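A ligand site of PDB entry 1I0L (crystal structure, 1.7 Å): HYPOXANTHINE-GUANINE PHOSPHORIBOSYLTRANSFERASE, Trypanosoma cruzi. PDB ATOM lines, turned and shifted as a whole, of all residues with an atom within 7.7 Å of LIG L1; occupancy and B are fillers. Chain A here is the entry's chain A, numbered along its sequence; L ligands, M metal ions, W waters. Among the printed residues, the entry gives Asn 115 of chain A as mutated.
N of Thr 116 is in hydrogen-bond range of O6 of LG2 L2 (3.1 Å).
The side-chain amide nitrogen (ND2) of Asn 115 lies within hydrogen-bond range of an oxygen (O8) of LG2 L2 (2.8 Å).
N of Val 165 lies within hydrogen-bond range of O1 of LIG L1 (2.9 Å).
O1 of LIG L1 is in hydrogen-bond range of NZ of Lys 143, at 3.0 Å.
The backbone carbonyl oxygen (O) of Val 165 sits close to a nitrogen (N2) of LIG L1, at 2.7 Å.
The guanidinium group (NH2) of Arg 177 lies within salt-bridge range of an oxygen (O13) of LG2 L2, at 3.5 Å.
The side-chain hydroxyl of Thr 116 sits at hydrogen-bond distance from an oxygen (O6) of LG2 L2 (2.8 Å).
O1 of LIG L1 is in hydrogen-bond range of O of Ala 163 (3.4 Å).
O of Phe 164 sits at hydrogen-bond distance from N of Leu 185, at 3.0 Å.
O of Val 114 lies within hydrogen-bond range of N of Lys 143, 2.9 Å away.
The side-chain carboxylate of Asp 171 lies within salt-bridge range of the guanidinium group of Arg 177.
The side-chain amino group of Lys 143 is in hydrogen-bond range of the backbone carbonyl oxygen of Ala 163 (2.8 Å).
Water W2 lies within hydrogen-bond range of N1 of LIG L1 and O2 of LG2 L2.
Water W4 lies within hydrogen-bond range of O8 of LG2 L2 (2.7 Å) and N4 of LIG L1 (3.4 Å).
Water W3 bridges the backbone carbonyl oxygen of Asp 171 and a nitrogen (N1) of LIG L1.
An oxygen (O8) of LG2 L2 lies within hydrogen-bond range of a nitrogen (N3) of LIG L1 (3.5 Å).
CD1 of Ile 113 touches C4 of LIG L1, at 3.6 Å.
Phe 164 touches LIG L1 (CA to O1, 3.3 Å).
CD2 of Leu 170 touches C3 of LIG L1, 3.7 Å away.
O of Asp 171 touches C3 of LIG L1, 3.7 Å away.
The nearest printed residue that does not touch LIG L1 is Asn 115 (4.5 Å).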
ATOM      1  N   ASP A 112     -10.232  35.811  19.642  1.00  0.00           N
ATOM      2  CA  ASP A 112      -8.928  35.217  19.832  1.00  0.00           C
ATOM      3  C   ASP A 112      -8.257  34.706  18.570  1.00  0.00           C
ATOM      4  O   ASP A 112      -7.033  34.662  18.482  1.00  0.00           O
ATOM      5  CB  ASP A 112      -8.860  34.224  21.020  1.00  0.00           C
ATOM      6  CG  ASP A 112      -9.703  33.008  20.835  1.00  0.00           C
ATOM      7  OD1 ASP A 112     -10.672  33.028  20.049  1.00  0.00           O
ATOM      8  OD2 ASP A 112      -9.399  32.005  21.529  1.00  0.00           O
ATOM      9  N   ILE A 113      -9.048  34.439  17.538  1.00  0.00           N
ATOM     10  CA  ILE A 113      -8.436  33.981  16.305  1.00  0.00           C
ATOM     11  C   ILE A 113      -9.284  34.376  15.090  1.00  0.00           C
ATOM     12  O   ILE A 113     -10.509  34.411  15.174  1.00  0.00           O
ATOM     13  CB  ILE A 113      -8.153  32.429  16.315  1.00  0.00           C
ATOM     14  CG1 ILE A 113      -7.150  32.050  15.206  1.00  0.00           C
ATOM     15  CG2 ILE A 113      -9.422  31.631  16.111  1.00  0.00           C
ATOM     16  CD1 ILE A 113      -6.602  30.610  15.314  1.00  0.00           C
ATOM     17  N   VAL A 114      -8.604  34.834  14.023  1.00  0.00           N
ATOM     18  CA  VAL A 114      -9.300  35.134  12.775  1.00  0.00           C
ATOM     19  C   VAL A 114      -8.551  34.377  11.689  1.00  0.00           C
ATOM     20  O   VAL A 114      -7.330  34.348  11.666  1.00  0.00           O
ATOM     21  CB  VAL A 114      -9.387  36.637  12.497  1.00  0.00           C
ATOM     22  CG1 VAL A 114      -8.018  37.239  12.418  1.00  0.00           C
ATOM     23  CG2 VAL A 114     -10.242  36.886  11.241  1.00  0.00           C
ATOM     24  N   ASN A 115      -9.331  33.624  10.915  1.00  0.00           N
ATOM     25  CA  ASN A 115      -8.854  32.777   9.833  1.00  0.00           C
ATOM     26  C   ASN A 115      -9.702  33.088   8.583  1.00  0.00           C
ATOM     27  O   ASN A 115      -9.361  34.021   7.830  1.00  0.00           O
ATOM     28  CB  ASN A 115      -8.975  31.313  10.249  1.00  0.00           C
ATOM     29  CG  ASN A 115      -8.442  30.357   9.221  1.00  0.00           C
ATOM     30  OD1 ASN A 115      -7.508  30.682   8.504  1.00  0.00           O
ATOM     31  ND2 ASN A 115      -9.024  29.167   9.133  1.00  0.00           N
ATOM     32  N   THR A 116     -10.828  32.382   8.395  1.00  0.00           N
ATOM     33  CA  THR A 116     -11.722  32.645   7.233  1.00  0.00           C
ATOM     34  C   THR A 116     -12.364  34.018   7.337  1.00  0.00           C
ATOM     35  O   THR A 116     -12.665  34.651   6.310  1.00  0.00           O
ATOM     36  CB  THR A 116     -12.875  31.631   7.106  1.00  0.00           C
ATOM     37  OG1 THR A 116     -13.740  31.739   8.244  1.00  0.00           O
ATOM     38  CG2 THR A 116     -12.373  30.224   6.953  1.00  0.00           C
ATOM     39  N   LEU A 141      -4.675  36.011  17.555  1.00  0.00           N
ATOM     40  CA  LEU A 141      -3.946  35.348  16.475  1.00  0.00           C
ATOM     41  C   LEU A 141      -4.597  35.528  15.103  1.00  0.00           C
ATOM     42  O   LEU A 141      -5.824  35.439  14.990  1.00  0.00           O
ATOM     43  CB  LEU A 141      -3.827  33.855  16.785  1.00  0.00           C
ATOM     44  CG  LEU A 141      -3.240  33.483  18.152  1.00  0.00           C
ATOM     45  CD1 LEU A 141      -3.175  31.979  18.226  1.00  0.00           C
ATOM     46  CD2 LEU A 141      -1.857  34.072  18.338  1.00  0.00           C
ATOM     47  N   LYS A 143      -4.504  34.220  11.067  1.00  0.00           N
ATOM     48  CA  LYS A 143      -4.040  33.317  10.015  1.00  0.00           C
ATOM     49  C   LYS A 143      -4.357  34.128   8.742  1.00  0.00           C
ATOM     50  O   LYS A 143      -5.387  33.932   8.085  1.00  0.00           O
ATOM     51  CB  LYS A 143      -4.801  32.014  10.014  1.00  0.00           C
ATOM     52  CG  LYS A 143      -4.445  31.087  11.150  1.00  0.00           C
ATOM     53  CD  LYS A 143      -5.147  29.750  10.998  1.00  0.00           C
ATOM     54  CE  LYS A 143      -4.786  28.809  12.143  1.00  0.00           C
ATOM     55  NZ  LYS A 143      -5.580  27.552  12.109  1.00  0.00           N
ATOM     56  N   ILE A 160       0.013  33.970  12.443  1.00  0.00           N
ATOM     57  CA  ILE A 160       0.430  32.585  12.519  1.00  0.00           C
ATOM     58  C   ILE A 160       0.065  31.861  11.238  1.00  0.00           C
ATOM     59  O   ILE A 160      -0.797  32.313  10.484  1.00  0.00           O
ATOM     60  CB  ILE A 160      -0.230  31.831  13.724  1.00  0.00           C
ATOM     61  CG1 ILE A 160      -1.753  31.974  13.677  1.00  0.00           C
ATOM     62  CG2 ILE A 160       0.304  32.365  15.048  1.00  0.00           C
ATOM     63  CD1 ILE A 160      -2.528  30.776  14.229  1.00  0.00           C
ATOM     64  N   PRO A 161       0.762  30.763  10.942  1.00  0.00           N
ATOM     65  CA  PRO A 161       0.520  29.949   9.747  1.00  0.00           C
ATOM     66  C   PRO A 161      -0.727  29.072   9.916  1.00  0.00           C
ATOM     67  O   PRO A 161      -1.387  29.119  10.966  1.00  0.00           O
ATOM     68  CB  PRO A 161       1.783  29.079   9.692  1.00  0.00           C
ATOM     69  CG  PRO A 161       2.144  28.934  11.134  1.00  0.00           C
ATOM     70  CD  PRO A 161       1.989  30.331  11.628  1.00  0.00           C
ATOM     71  N   ASN A 162      -1.014  28.240   8.918  1.00  0.00           N
ATOM     72  CA  ASN A 162      -2.182  27.373   9.013  1.00  0.00           C
ATOM     73  C   ASN A 162      -1.900  26.084   9.767  1.00  0.00           C
ATOM     74  O   ASN A 162      -1.483  25.081   9.189  1.00  0.00           O
ATOM     75  CB  ASN A 162      -2.746  27.007   7.648  1.00  0.00           C
ATOM     76  CG  ASN A 162      -3.930  26.062   7.773  1.00  0.00           C
ATOM     77  OD1 ASN A 162      -3.817  24.862   7.508  1.00  0.00           O
ATOM     78  ND2 ASN A 162      -5.050  26.594   8.251  1.00  0.00           N
ATOM     79  N   ALA A 163      -2.103  26.129  11.061  1.00  0.00           N
ATOM     80  CA  ALA A 163      -1.902  24.959  11.896  1.00  0.00           C
ATOM     81  C   ALA A 163      -2.978  25.118  12.959  1.00  0.00           C
ATOM     82  O   ALA A 163      -3.398  26.245  13.264  1.00  0.00           O
ATOM     83  CB  ALA A 163      -0.521  25.015  12.529  1.00  0.00           C
ATOM     84  N   PHE A 164      -3.518  24.015  13.467  1.00  0.00           N
ATOM     85  CA  PHE A 164      -4.546  24.132  14.477  1.00  0.00           C
ATOM     86  C   PHE A 164      -3.844  24.391  15.784  1.00  0.00           C
ATOM     87  O   PHE A 164      -3.002  23.606  16.196  1.00  0.00           O
ATOM     88  CB  PHE A 164      -5.392  22.851  14.551  1.00  0.00           C
ATOM     89  CG  PHE A 164      -6.761  23.084  15.148  1.00  0.00           C
ATOM     90  CD1 PHE A 164      -7.781  23.624  14.361  1.00  0.00           C
ATOM     91  CD2 PHE A 164      -7.013  22.830  16.483  1.00  0.00           C
ATOM     92  CE1 PHE A 164      -9.031  23.929  14.917  1.00  0.00           C
ATOM     93  CE2 PHE A 164      -8.254  23.133  17.042  1.00  0.00           C
ATOM     94  CZ  PHE A 164      -9.260  23.684  16.255  1.00  0.00           C
ATOM     95  N   VAL A 165      -4.110  25.530  16.377  1.00  0.00           N
ATOM     96  CA  VAL A 165      -3.499  25.925  17.645  1.00  0.00           C
ATOM     97  C   VAL A 165      -4.531  25.791  18.788  1.00  0.00           C
ATOM     98  O   VAL A 165      -5.732  25.991  18.582  1.00  0.00           O
ATOM     99  CB  VAL A 165      -2.919  27.379  17.592  1.00  0.00           C
ATOM    100  CG1 VAL A 165      -1.850  27.481  16.527  1.00  0.00           C
ATOM    101  CG2 VAL A 165      -4.007  28.393  17.306  1.00  0.00           C
ATOM    102  N   ILE A 166      -4.047  25.488  19.987  1.00  0.00           N
ATOM    103  CA  ILE A 166      -4.911  25.300  21.157  1.00  0.00           C
ATOM    104  C   ILE A 166      -4.252  25.975  22.352  1.00  0.00           C
ATOM    105  O   ILE A 166      -3.043  26.240  22.325  1.00  0.00           O
ATOM    106  CB  ILE A 166      -5.096  23.783  21.494  1.00  0.00           C
ATOM    107  CG1 ILE A 166      -3.722  23.080  21.505  1.00  0.00           C
ATOM    108  CG2 ILE A 166      -6.090  23.115  20.538  1.00  0.00           C
ATOM    109  CD1 ILE A 166      -3.765  21.626  21.821  1.00  0.00           C
ATOM    110  N   GLY A 167      -5.021  26.216  23.402  1.00  0.00           N
ATOM    111  CA  GLY A 167      -4.491  26.847  24.597  1.00  0.00           C
ATOM    112  C   GLY A 167      -4.871  28.300  24.616  1.00  0.00           C
ATOM    113  O   GLY A 167      -5.328  28.840  23.602  1.00  0.00           O
ATOM    114  N   GLY A 169      -7.491  29.870  25.685  1.00  0.00           N
ATOM    115  CA  GLY A 169      -8.859  30.140  25.231  1.00  0.00           C
ATOM    116  C   GLY A 169      -9.244  29.325  24.009  1.00  0.00           C
ATOM    117  O   GLY A 169     -10.411  28.973  23.829  1.00  0.00           O
ATOM    118  N   LEU A 170      -8.258  28.945  23.216  1.00  0.00           N
ATOM    119  CA  LEU A 170      -8.496  28.181  22.006  1.00  0.00           C
ATOM    120  C   LEU A 170      -8.650  26.716  22.321  1.00  0.00           C
ATOM    121  O   LEU A 170      -7.824  26.124  22.998  1.00  0.00           O
ATOM    122  CB  LEU A 170      -7.328  28.366  21.027  1.00  0.00           C
ATOM    123  CG  LEU A 170      -7.181  29.804  20.542  1.00  0.00           C
ATOM    124  CD1 LEU A 170      -5.757  30.063  20.119  1.00  0.00           C
ATOM    125  CD2 LEU A 170      -8.142  30.040  19.394  1.00  0.00           C
ATOM    126  N   ASP A 171      -9.639  26.112  21.682  1.00  0.00           N
ATOM    127  CA  ASP A 171      -9.930  24.699  21.924  1.00  0.00           C
ATOM    128  C   ASP A 171      -9.983  23.803  20.719  1.00  0.00           C
ATOM    129  O   ASP A 171     -10.020  24.232  19.561  1.00  0.00           O
ATOM    130  CB  ASP A 171     -11.334  24.589  22.563  1.00  0.00           C
ATOM    131  CG  ASP A 171     -12.458  24.883  21.560  1.00  0.00           C
ATOM    132  OD1 ASP A 171     -12.492  26.002  20.981  1.00  0.00           O
ATOM    133  OD2 ASP A 171     -13.315  24.006  21.342  1.00  0.00           O
ATOM    134  N   TYR A 172      -9.978  22.518  21.021  1.00  0.00           N
ATOM    135  CA  TYR A 172     -10.227  21.534  20.026  1.00  0.00           C
ATOM    136  C   TYR A 172     -11.294  20.711  20.742  1.00  0.00           C
ATOM    137  O   TYR A 172     -11.029  20.122  21.794  1.00  0.00           O
ATOM    138  CB  TYR A 172      -9.055  20.622  19.704  1.00  0.00           C
ATOM    139  CG  TYR A 172      -9.569  19.537  18.795  1.00  0.00           C
ATOM    140  CD1 TYR A 172     -10.170  19.879  17.576  1.00  0.00           C
ATOM    141  CD2 TYR A 172      -9.700  18.213  19.240  1.00  0.00           C
ATOM    142  CE1 TYR A 172     -10.902  18.973  16.858  1.00  0.00           C
ATOM    143  CE2 TYR A 172     -10.441  17.290  18.510  1.00  0.00           C
ATOM    144  CZ  TYR A 172     -11.047  17.693  17.327  1.00  0.00           C
ATOM    145  OH  TYR A 172     -11.896  16.865  16.630  1.00  0.00           O
ATOM    146  N   ARG A 177      -8.666  24.683  26.315  1.00  0.00           N
ATOM    147  CA  ARG A 177      -8.775  26.133  26.447  1.00  0.00           C
ATOM    148  C   ARG A 177      -7.949  26.653  27.627  1.00  0.00           C
ATOM    149  O   ARG A 177      -7.454  27.796  27.592  1.00  0.00           O
ATOM    150  CB  ARG A 177     -10.221  26.557  26.689  1.00  0.00           C
ATOM    151  CG  ARG A 177     -11.250  26.100  25.696  1.00  0.00           C
ATOM    152  CD  ARG A 177     -12.502  26.962  25.825  1.00  0.00           C
ATOM    153  NE  ARG A 177     -13.564  26.469  24.968  1.00  0.00           N
ATOM    154  CZ  ARG A 177     -13.809  26.908  23.732  1.00  0.00           C
ATOM    155  NH1 ARG A 177     -13.040  27.870  23.198  1.00  0.00           N
ATOM    156  NH2 ARG A 177     -14.778  26.347  23.014  1.00  0.00           N
ATOM    157  N   VAL A 183      -0.112  26.367  21.791  1.00  0.00           N
ATOM    158  CA  VAL A 183       0.627  25.293  21.179  1.00  0.00           C
ATOM    159  C   VAL A 183      -0.080  24.789  19.911  1.00  0.00           C
ATOM    160  O   VAL A 183      -1.227  25.163  19.626  1.00  0.00           O
ATOM    161  CB  VAL A 183       0.864  24.089  22.198  1.00  0.00           C
ATOM    162  CG1 VAL A 183       1.461  24.602  23.521  1.00  0.00           C
ATOM    163  CG2 VAL A 183      -0.410  23.319  22.447  1.00  0.00           C
ATOM    164  N   LEU A 185      -1.570  21.704  17.965  1.00  0.00           N
ATOM    165  CA  LEU A 185      -2.049  20.364  18.238  1.00  0.00           C
ATOM    166  C   LEU A 185      -1.476  19.395  17.190  1.00  0.00           C
ATOM    167  O   LEU A 185      -1.396  19.728  16.003  1.00  0.00           O
ATOM    168  CB  LEU A 185      -3.579  20.345  18.191  1.00  0.00           C
ATOM    169  CG  LEU A 185      -4.310  19.005  18.383  1.00  0.00           C
ATOM    170  CD1 LEU A 185      -4.047  18.445  19.781  1.00  0.00           C
ATOM    171  CD2 LEU A 185      -5.786  19.242  18.112  1.00  0.00           C
ATOM    172  N   TYR A 190      -5.635  15.783  15.624  1.00  0.00           N
ATOM    173  CA  TYR A 190      -6.742  16.538  15.075  1.00  0.00           C
ATOM    174  C   TYR A 190      -7.513  15.698  14.042  1.00  0.00           C
ATOM    175  O   TYR A 190      -8.745  15.606  14.093  1.00  0.00           O
ATOM    176  CB  TYR A 190      -6.239  17.840  14.427  1.00  0.00           C
ATOM    177  CG  TYR A 190      -7.366  18.680  13.880  1.00  0.00           C
ATOM    178  CD1 TYR A 190      -7.980  19.659  14.672  1.00  0.00           C
ATOM    179  CD2 TYR A 190      -7.885  18.454  12.597  1.00  0.00           C
ATOM    180  CE1 TYR A 190      -9.081  20.383  14.197  1.00  0.00           C
ATOM    181  CE2 TYR A 190      -8.986  19.178  12.122  1.00  0.00           C
ATOM    182  CZ  TYR A 190      -9.577  20.130  12.926  1.00  0.00           C
ATOM    183  OH  TYR A 190     -10.690  20.807  12.485  1.00  0.00           O
HETATM  184  C1  LIG L   1     -10.595  28.197  14.564  1.00  0.00           C
HETATM  185  C2  LIG L   1      -9.684  27.686  15.487  1.00  0.00           C
HETATM  186  N1  LIG L   1      -9.918  27.373  16.782  1.00  0.00           N
HETATM  187  C3  LIG L   1      -8.778  26.941  17.387  1.00  0.00           C
HETATM  188  N2  LIG L   1      -7.568  26.833  16.750  1.00  0.00           N
HETATM  189  C4  LIG L   1      -7.334  27.127  15.422  1.00  0.00           C
HETATM  190  O1  LIG L   1      -6.259  26.908  14.921  1.00  0.00           O
HETATM  191  C5  LIG L   1      -8.479  27.573  14.808  1.00  0.00           C
HETATM  192  N3  LIG L   1      -8.680  28.002  13.519  1.00  0.00           N
HETATM  193  N4  LIG L   1      -9.925  28.351  13.448  1.00  0.00           N
HETATM  194  C1  LG2 L   2     -13.606  29.387  16.148  1.00  0.00           C
HETATM  195  C2  LG2 L   2     -12.515  30.302  16.071  1.00  0.00           C
HETATM  196  C3  LG2 L   2     -13.070  31.358  15.115  1.00  0.00           C
HETATM  197  C4  LG2 L   2     -14.101  30.579  14.297  1.00  0.00           C
HETATM  198  C5  LG2 L   2     -13.646  30.541  12.860  1.00  0.00           C
HETATM  199  O1  LG2 L   2     -14.668  29.835  17.064  1.00  0.00           O
HETATM  200  O2  LG2 L   2     -12.321  30.587  17.440  1.00  0.00           O
HETATM  201  O3  LG2 L   2     -13.580  32.442  15.836  1.00  0.00           O
HETATM  202  O4  LG2 L   2     -13.957  29.210  14.828  1.00  0.00           O
HETATM  203  O5  LG2 L   2     -13.086  29.308  12.366  1.00  0.00           O
HETATM  204  P1  LG2 L   2     -12.368  29.268  10.858  1.00  0.00           P
HETATM  205  O6  LG2 L   2     -12.371  30.720  10.494  1.00  0.00           O
HETATM  206  O7  LG2 L   2     -13.253  28.362  10.110  1.00  0.00           O
HETATM  207  O8  LG2 L   2     -11.037  28.633  11.045  1.00  0.00           O
HETATM  208  P2  LG2 L   2     -15.431  28.611  17.732  1.00  0.00           P
HETATM  209  O9  LG2 L   2     -16.477  28.205  16.823  1.00  0.00           O
HETATM  210  O10 LG2 L   2     -14.439  27.561  17.870  1.00  0.00           O
HETATM  211  O11 LG2 L   2     -15.932  29.217  19.000  1.00  0.00           O
HETATM  212  P3  LG2 L   2     -15.269  29.177  20.353  1.00  0.00           P
HETATM  213  O12 LG2 L   2     -14.341  28.036  20.421  1.00  0.00           O
HETATM  214  O13 LG2 L   2     -16.325  29.077  21.413  1.00  0.00           O
HETATM  215  O14 LG2 L   2     -14.604  30.475  20.649  1.00  0.00           O
HETATM  216 MG    MG M   1     -13.346  26.812  19.314  1.00  0.00          MG
HETATM  217  O   HOH W   1     -12.835  25.710  15.517  1.00  0.00           O
HETATM  218  O   HOH W   2     -11.665  27.895  19.020  1.00  0.00           O
HETATM  219  O   HOH W   3     -12.413  25.358  18.055  1.00  0.00           O
HETATM  220  O   HOH W   4     -10.042  26.089  10.895  1.00  0.00           O
